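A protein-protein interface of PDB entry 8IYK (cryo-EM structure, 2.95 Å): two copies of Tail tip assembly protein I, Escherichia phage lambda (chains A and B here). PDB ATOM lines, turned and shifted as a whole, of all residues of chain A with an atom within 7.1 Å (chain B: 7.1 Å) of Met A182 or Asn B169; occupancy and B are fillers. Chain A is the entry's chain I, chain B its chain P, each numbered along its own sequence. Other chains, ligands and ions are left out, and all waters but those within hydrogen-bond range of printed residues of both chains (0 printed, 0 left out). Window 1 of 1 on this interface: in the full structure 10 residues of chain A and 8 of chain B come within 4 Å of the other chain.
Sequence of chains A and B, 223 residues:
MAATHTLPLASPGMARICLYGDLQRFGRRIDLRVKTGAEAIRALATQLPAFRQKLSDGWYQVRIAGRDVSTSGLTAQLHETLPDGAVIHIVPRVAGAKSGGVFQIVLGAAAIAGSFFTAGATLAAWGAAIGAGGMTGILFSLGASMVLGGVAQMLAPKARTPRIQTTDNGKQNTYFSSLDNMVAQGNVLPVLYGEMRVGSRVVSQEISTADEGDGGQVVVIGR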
ATOM      1  N   SER A 178     -25.040  -5.419 -24.440  1.00  0.00           N
ATOM      2  CA  SER A 178     -24.336  -6.210 -23.440  1.00  0.00           C
ATOM      3  C   SER A 178     -25.258  -7.320 -22.969  1.00  0.00           C
ATOM      4  O   SER A 178     -26.426  -7.067 -22.660  1.00  0.00           O
ATOM      5  CB  SER A 178     -23.896  -5.343 -22.257  1.00  0.00           C
ATOM      6  OG  SER A 178     -23.083  -6.079 -21.359  1.00  0.00           O
ATOM      7  N   LEU A 179     -24.736  -8.544 -22.917  1.00  0.00           N
ATOM      8  CA  LEU A 179     -25.474  -9.698 -22.422  1.00  0.00           C
ATOM      9  C   LEU A 179     -24.867 -10.242 -21.134  1.00  0.00           C
ATOM     10  O   LEU A 179     -24.891 -11.450 -20.889  1.00  0.00           O
ATOM     11  CB  LEU A 179     -25.533 -10.795 -23.483  1.00  0.00           C
ATOM     12  CG  LEU A 179     -26.203 -10.445 -24.810  1.00  0.00           C
ATOM     13  CD1 LEU A 179     -25.932 -11.529 -25.834  1.00  0.00           C
ATOM     14  CD2 LEU A 179     -27.690 -10.255 -24.620  1.00  0.00           C
ATOM     15  N   ASP A 180     -24.318  -9.360 -20.304  1.00  0.00           N
ATOM     16  CA  ASP A 180     -23.642  -9.744 -19.077  1.00  0.00           C
ATOM     17  C   ASP A 180     -24.316  -9.085 -17.883  1.00  0.00           C
ATOM     18  O   ASP A 180     -24.969  -8.045 -18.005  1.00  0.00           O
ATOM     19  CB  ASP A 180     -22.160  -9.349 -19.109  1.00  0.00           C
ATOM     20  CG  ASP A 180     -21.534  -9.534 -20.477  1.00  0.00           C
ATOM     21  OD1 ASP A 180     -21.891 -10.507 -21.173  1.00  0.00           O
ATOM     22  OD2 ASP A 180     -20.684  -8.703 -20.859  1.00  0.00           O
ATOM     23  N   ASN A 181     -24.149  -9.707 -16.718  1.00  0.00           N
ATOM     24  CA  ASN A 181     -24.628  -9.160 -15.450  1.00  0.00           C
ATOM     25  C   ASN A 181     -23.429  -8.512 -14.766  1.00  0.00           C
ATOM     26  O   ASN A 181     -22.738  -9.131 -13.958  1.00  0.00           O
ATOM     27  CB  ASN A 181     -25.264 -10.246 -14.592  1.00  0.00           C
ATOM     28  CG  ASN A 181     -26.538 -10.798 -15.199  1.00  0.00           C
ATOM     29  OD1 ASN A 181     -27.525 -10.084 -15.354  1.00  0.00           O
ATOM     30  ND2 ASN A 181     -26.520 -12.078 -15.547  1.00  0.00           N
ATOM     31  N   MET A 182     -23.187  -7.247 -15.099  1.00  0.00           N
ATOM     32  CA  MET A 182     -21.974  -6.554 -14.700  1.00  0.00           C
ATOM     33  C   MET A 182     -22.062  -6.071 -13.254  1.00  0.00           C
ATOM     34  O   MET A 182     -23.119  -6.086 -12.621  1.00  0.00           O
ATOM     35  CB  MET A 182     -21.706  -5.376 -15.633  1.00  0.00           C
ATOM     36  CG  MET A 182     -21.773  -5.729 -17.108  1.00  0.00           C
ATOM     37  SD  MET A 182     -22.261  -4.332 -18.135  1.00  0.00           S
ATOM     38  CE  MET A 182     -23.982  -4.155 -17.677  1.00  0.00           C
ATOM     39  N   VAL A 183     -20.913  -5.638 -12.731  1.00  0.00           N
ATOM     40  CA  VAL A 183     -20.854  -5.063 -11.395  1.00  0.00           C
ATOM     41  C   VAL A 183     -21.486  -3.678 -11.413  1.00  0.00           C
ATOM     42  O   VAL A 183     -21.312  -2.906 -12.366  1.00  0.00           O
ATOM     43  CB  VAL A 183     -19.395  -5.020 -10.906  1.00  0.00           C
ATOM     44  CG1 VAL A 183     -19.236  -4.084  -9.721  1.00  0.00           C
ATOM     45  CG2 VAL A 183     -18.917  -6.417 -10.548  1.00  0.00           C
ATOM     46  N   ALA A 184     -22.229  -3.354 -10.358  1.00  0.00           N
ATOM     47  CA  ALA A 184     -23.048  -2.147 -10.305  1.00  0.00           C
ATOM     48  C   ALA A 184     -22.558  -1.157  -9.252  1.00  0.00           C
ATOM     49  O   ALA A 184     -23.352  -0.587  -8.506  1.00  0.00           O
ATOM     50  CB  ALA A 184     -24.507  -2.504 -10.044  1.00  0.00           C
ATOM     51  N   GLN A 185     -21.248  -0.938  -9.178  1.00  0.00           N
ATOM     52  CA  GLN A 185     -20.665   0.019  -8.245  1.00  0.00           C
ATOM     53  C   GLN A 185     -19.868   1.049  -9.034  1.00  0.00           C
ATOM     54  O   GLN A 185     -18.887   0.700  -9.699  1.00  0.00           O
ATOM     55  CB  GLN A 185     -19.777  -0.687  -7.220  1.00  0.00           C
ATOM     56  CG  GLN A 185     -18.706   0.194  -6.602  1.00  0.00           C
ATOM     57  CD  GLN A 185     -19.052   0.641  -5.197  1.00  0.00           C
ATOM     58  OE1 GLN A 185     -19.317  -0.181  -4.322  1.00  0.00           O
ATOM     59  NE2 GLN A 185     -19.044   1.948  -4.972  1.00  0.00           N
ATOM     60  N   ASN A 187     -20.598   2.824 -11.790  1.00  0.00           N
ATOM     61  CA  ASN A 187     -20.530   2.266 -13.129  1.00  0.00           C
ATOM     62  C   ASN A 187     -21.521   2.845 -14.131  1.00  0.00           C
ATOM     63  O   ASN A 187     -21.512   2.405 -15.282  1.00  0.00           O
ATOM     64  CB  ASN A 187     -20.735   0.749 -13.060  1.00  0.00           C
ATOM     65  CG  ASN A 187     -19.473  -0.018 -13.341  1.00  0.00           C
ATOM     66  OD1 ASN A 187     -18.594   0.447 -14.063  1.00  0.00           O
ATOM     67  ND2 ASN A 187     -19.367  -1.202 -12.758  1.00  0.00           N
ATOM     68  N   VAL A 188     -22.362   3.803 -13.722  1.00  0.00           N
ATOM     69  CA  VAL A 188     -23.500   4.395 -14.442  1.00  0.00           C
ATOM     70  C   VAL A 188     -24.481   3.297 -14.844  1.00  0.00           C
ATOM     71  O   VAL A 188     -24.079   2.195 -15.229  1.00  0.00           O
ATOM     72  CB  VAL A 188     -23.098   5.271 -15.654  1.00  0.00           C
ATOM     73  CG1 VAL A 188     -22.182   6.416 -15.224  1.00  0.00           C
ATOM     74  CG2 VAL A 188     -22.583   4.498 -16.862  1.00  0.00           C
ATOM     75  N   PRO A 190     -27.284   1.725 -17.155  1.00  0.00           N
ATOM     76  CA  PRO A 190     -27.402   1.738 -18.572  1.00  0.00           C
ATOM     77  C   PRO A 190     -28.663   2.397 -19.108  1.00  0.00           C
ATOM     78  O   PRO A 190     -29.524   2.528 -18.345  1.00  0.00           O
ATOM     79  CB  PRO A 190     -27.359   0.239 -18.794  1.00  0.00           C
ATOM     80  CG  PRO A 190     -27.930  -0.378 -17.576  1.00  0.00           C
ATOM     81  CD  PRO A 190     -27.235   0.423 -16.516  1.00  0.00           C
ATOM     82  N   GLY A 199     -28.423  -7.524 -20.562  1.00  0.00           N
ATOM     83  CA  GLY A 199     -27.939  -8.064 -19.311  1.00  0.00           C
ATOM     84  C   GLY A 199     -28.512  -7.258 -18.168  1.00  0.00           C
ATOM     85  O   GLY A 199     -29.715  -6.983 -18.159  1.00  0.00           O
ATOM     86  N   SER A 200     -27.676  -6.852 -17.214  1.00  0.00           N
ATOM     87  CA  SER A 200     -28.148  -6.055 -16.088  1.00  0.00           C
ATOM     88  C   SER A 200     -26.954  -5.616 -15.252  1.00  0.00           C
ATOM     89  O   SER A 200     -25.828  -6.087 -15.436  1.00  0.00           O
ATOM     90  CB  SER A 200     -29.134  -6.827 -15.215  1.00  0.00           C
ATOM     91  OG  SER A 200     -28.818  -8.207 -15.185  1.00  0.00           O
ATOM     92  N   ARG A 201     -27.222  -4.700 -14.329  1.00  0.00           N
ATOM     93  CA  ARG A 201     -26.292  -4.317 -13.272  1.00  0.00           C
ATOM     94  C   ARG A 201     -26.870  -4.875 -11.977  1.00  0.00           C
ATOM     95  O   ARG A 201     -27.843  -4.337 -11.442  1.00  0.00           O
ATOM     96  CB  ARG A 201     -26.123  -2.804 -13.205  1.00  0.00           C
ATOM     97  CG  ARG A 201     -25.622  -2.163 -14.483  1.00  0.00           C
ATOM     98  CD  ARG A 201     -24.568  -1.115 -14.183  1.00  0.00           C
ATOM     99  NE  ARG A 201     -23.939  -0.607 -15.395  1.00  0.00           N
ATOM    100  CZ  ARG A 201     -22.692  -0.872 -15.759  1.00  0.00           C
ATOM    101  NH1 ARG A 201     -21.909  -1.647 -15.028  1.00  0.00           N
ATOM    102  NH2 ARG A 201     -22.219  -0.345 -16.884  1.00  0.00           N
ATOM    103  N   VAL A 202     -26.277  -5.959 -11.482  1.00  0.00           N
ATOM    104  CA  VAL A 202     -26.840  -6.668 -10.338  1.00  0.00           C
ATOM    105  C   VAL A 202     -26.794  -5.763  -9.114  1.00  0.00           C
ATOM    106  O   VAL A 202     -25.721  -5.319  -8.691  1.00  0.00           O
ATOM    107  CB  VAL A 202     -26.092  -7.982 -10.087  1.00  0.00           C
ATOM    108  CG1 VAL A 202     -26.945  -8.925  -9.257  1.00  0.00           C
ATOM    109  CG2 VAL A 202     -25.712  -8.626 -11.403  1.00  0.00           C
ATOM    110  N   VAL A 203     -27.962  -5.490  -8.541  1.00  0.00           N
ATOM    111  CA  VAL A 203     -28.053  -4.637  -7.361  1.00  0.00           C
ATOM    112  C   VAL A 203     -28.011  -5.459  -6.080  1.00  0.00           C
ATOM    113  O   VAL A 203     -27.314  -5.101  -5.127  1.00  0.00           O
ATOM    114  CB  VAL A 203     -29.327  -3.771  -7.441  1.00  0.00           C
ATOM    115  CG1 VAL A 203     -29.839  -3.433  -6.051  1.00  0.00           C
ATOM    116  CG2 VAL A 203     -29.055  -2.506  -8.233  1.00  0.00           C
ATOM    117  N   ILE B 164      -9.985   1.254 -18.512  1.00  0.00           N
ATOM    118  CA  ILE B 164     -11.076   0.351 -18.175  1.00  0.00           C
ATOM    119  C   ILE B 164     -11.053  -0.844 -19.119  1.00  0.00           C
ATOM    120  O   ILE B 164     -11.059  -0.688 -20.348  1.00  0.00           O
ATOM    121  CB  ILE B 164     -12.422   1.088 -18.239  1.00  0.00           C
ATOM    122  CG1 ILE B 164     -12.620   1.941 -16.985  1.00  0.00           C
ATOM    123  CG2 ILE B 164     -13.568   0.100 -18.392  1.00  0.00           C
ATOM    124  CD1 ILE B 164     -13.252   3.286 -17.258  1.00  0.00           C
ATOM    125  N   GLN B 165     -11.027  -2.043 -18.548  1.00  0.00           N
ATOM    126  CA  GLN B 165     -10.954  -3.281 -19.310  1.00  0.00           C
ATOM    127  C   GLN B 165     -12.311  -3.970 -19.300  1.00  0.00           C
ATOM    128  O   GLN B 165     -12.929  -4.119 -18.241  1.00  0.00           O
ATOM    129  CB  GLN B 165      -9.887  -4.214 -18.737  1.00  0.00           C
ATOM    130  CG  GLN B 165      -8.570  -3.540 -18.410  1.00  0.00           C
ATOM    131  CD  GLN B 165      -7.380  -4.389 -18.805  1.00  0.00           C
ATOM    132  OE1 GLN B 165      -7.407  -5.612 -18.672  1.00  0.00           O
ATOM    133  NE2 GLN B 165      -6.327  -3.744 -19.294  1.00  0.00           N
ATOM    134  N   THR B 166     -12.769  -4.386 -20.483  1.00  0.00           N
ATOM    135  CA  THR B 166     -14.051  -5.073 -20.591  1.00  0.00           C
ATOM    136  C   THR B 166     -14.011  -6.471 -19.984  1.00  0.00           C
ATOM    137  O   THR B 166     -15.069  -7.017 -19.652  1.00  0.00           O
ATOM    138  CB  THR B 166     -14.483  -5.148 -22.056  1.00  0.00           C
ATOM    139  OG1 THR B 166     -14.173  -3.911 -22.708  1.00  0.00           O
ATOM    140  CG2 THR B 166     -15.982  -5.394 -22.165  1.00  0.00           C
ATOM    141  N   THR B 167     -12.821  -7.061 -19.831  1.00  0.00           N
ATOM    142  CA  THR B 167     -12.726  -8.373 -19.198  1.00  0.00           C
ATOM    143  C   THR B 167     -13.275  -8.335 -17.780  1.00  0.00           C
ATOM    144  O   THR B 167     -14.019  -9.232 -17.368  1.00  0.00           O
ATOM    145  CB  THR B 167     -11.279  -8.860 -19.194  1.00  0.00           C
ATOM    146  OG1 THR B 167     -11.050  -9.670 -18.034  1.00  0.00           O
ATOM    147  CG2 THR B 167     -10.325  -7.682 -19.176  1.00  0.00           C
ATOM    148  N   ASP B 168     -12.914  -7.307 -17.017  1.00  0.00           N
ATOM    149  CA  ASP B 168     -13.616  -7.030 -15.775  1.00  0.00           C
ATOM    150  C   ASP B 168     -15.045  -6.626 -16.101  1.00  0.00           C
ATOM    151  O   ASP B 168     -15.274  -5.764 -16.956  1.00  0.00           O
ATOM    152  CB  ASP B 168     -12.911  -5.921 -14.996  1.00  0.00           C
ATOM    153  CG  ASP B 168     -11.525  -6.322 -14.536  1.00  0.00           C
ATOM    154  OD1 ASP B 168     -11.262  -7.538 -14.430  1.00  0.00           O
ATOM    155  OD2 ASP B 168     -10.699  -5.423 -14.279  1.00  0.00           O
ATOM    156  N   ASN B 169     -16.011  -7.264 -15.437  1.00  0.00           N
ATOM    157  CA  ASN B 169     -17.413  -6.978 -15.717  1.00  0.00           C
ATOM    158  C   ASN B 169     -17.716  -5.502 -15.495  1.00  0.00           C
ATOM    159  O   ASN B 169     -18.058  -4.772 -16.432  1.00  0.00           O
ATOM    160  CB  ASN B 169     -18.308  -7.857 -14.845  1.00  0.00           C
ATOM    161  CG  ASN B 169     -18.946  -8.987 -15.624  1.00  0.00           C
ATOM    162  OD1 ASN B 169     -19.261  -8.843 -16.805  1.00  0.00           O
ATOM    163  ND2 ASN B 169     -19.141 -10.123 -14.965  1.00  0.00           N
ATOM    164  N   GLY B 170     -17.587  -5.045 -14.256  1.00  0.00           N
ATOM    165  CA  GLY B 170     -17.678  -3.633 -13.954  1.00  0.00           C
ATOM    166  C   GLY B 170     -16.719  -3.254 -12.850  1.00  0.00           C
ATOM    167  O   GLY B 170     -16.746  -2.127 -12.345  1.00  0.00           O
ATOM    168  N   LYS B 171     -15.866  -4.199 -12.467  1.00  0.00           N
ATOM    169  CA  LYS B 171     -14.938  -3.977 -11.369  1.00  0.00           C
ATOM    170  C   LYS B 171     -13.900  -2.930 -11.747  1.00  0.00           C
ATOM    171  O   LYS B 171     -13.386  -2.915 -12.868  1.00  0.00           O
ATOM    172  CB  LYS B 171     -14.248  -5.286 -10.989  1.00  0.00           C
ATOM    173  CG  LYS B 171     -13.616  -5.275  -9.612  1.00  0.00           C
ATOM    174  CD  LYS B 171     -14.185  -6.377  -8.736  1.00  0.00           C
ATOM    175  CE  LYS B 171     -13.286  -6.647  -7.543  1.00  0.00           C
ATOM    176  NZ  LYS B 171     -12.916  -5.394  -6.830  1.00  0.00           N
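O of Gly B170 is in hydrogen-bond range of ND2 of Asn A187 (2.8 Å).
No position is printed for both chains.
Among the printed residues, merely in contact across the chains: Val A183 with Gly B170, Asp A180 with Asn B169, Met A182 with Asn B169, Asn A181 with Asn B169 and Val A183 with Lys B171.
Of the 8 printed residues of chain B, 3 touch a printed residue of chain A. Of the 16 printed residues of chain A, 5 touch a printed residue of chain B. Hydrophobic or aromatic side chains of chain A that line the printed part of chain B: Met A182 and Val A183.
The side-chain hydroxyl (OG) of Ser A178 is in hydrogen-bond range of the side-chain sulfur (SD) of Met A182 (3.8 Å). The backbone carbonyl oxygen of Asp A180 is in hydrogen-bond range of the backbone NH of Ser A200 (3.1 Å). O of Ser A200 lies within hydrogen-bond range of N of Met A182. The backbone carbonyl oxygen (O) of Met A182 is in hydrogen-bond range of the backbone NH (N) of Val A202. O of Val A183 sits at hydrogen-bond distance from ND2 of Asn A187 (2.6 Å). The guanidinium group (NH1) of Arg A201 sits at hydrogen-bond distance from the backbone carbonyl oxygen (O) of Val A183 (3.0 Å).
Of chain B, only Asn B169 comes within 4 Å of Met A182. Printed residues of chain B within 4 Å of Asn A181: Asn B169 (3.9 Å). Of the printed residues of chain B, Asp A180 touches Asn B169 (3.7 Å). Ile B164 touches none of the printed residues of chain A. Ser A178 touches none of the printed residues of chain B. The nearest residue of chain B that does not touch Met A182 is Gly B170 (4.4 Å). The nearest residue of chain A that does not touch Asn B169 is Val A183 (4.02 Å). The nearest printed residue of chain B that does not touch Asp A180 is Thr B166 (5.9 Å).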
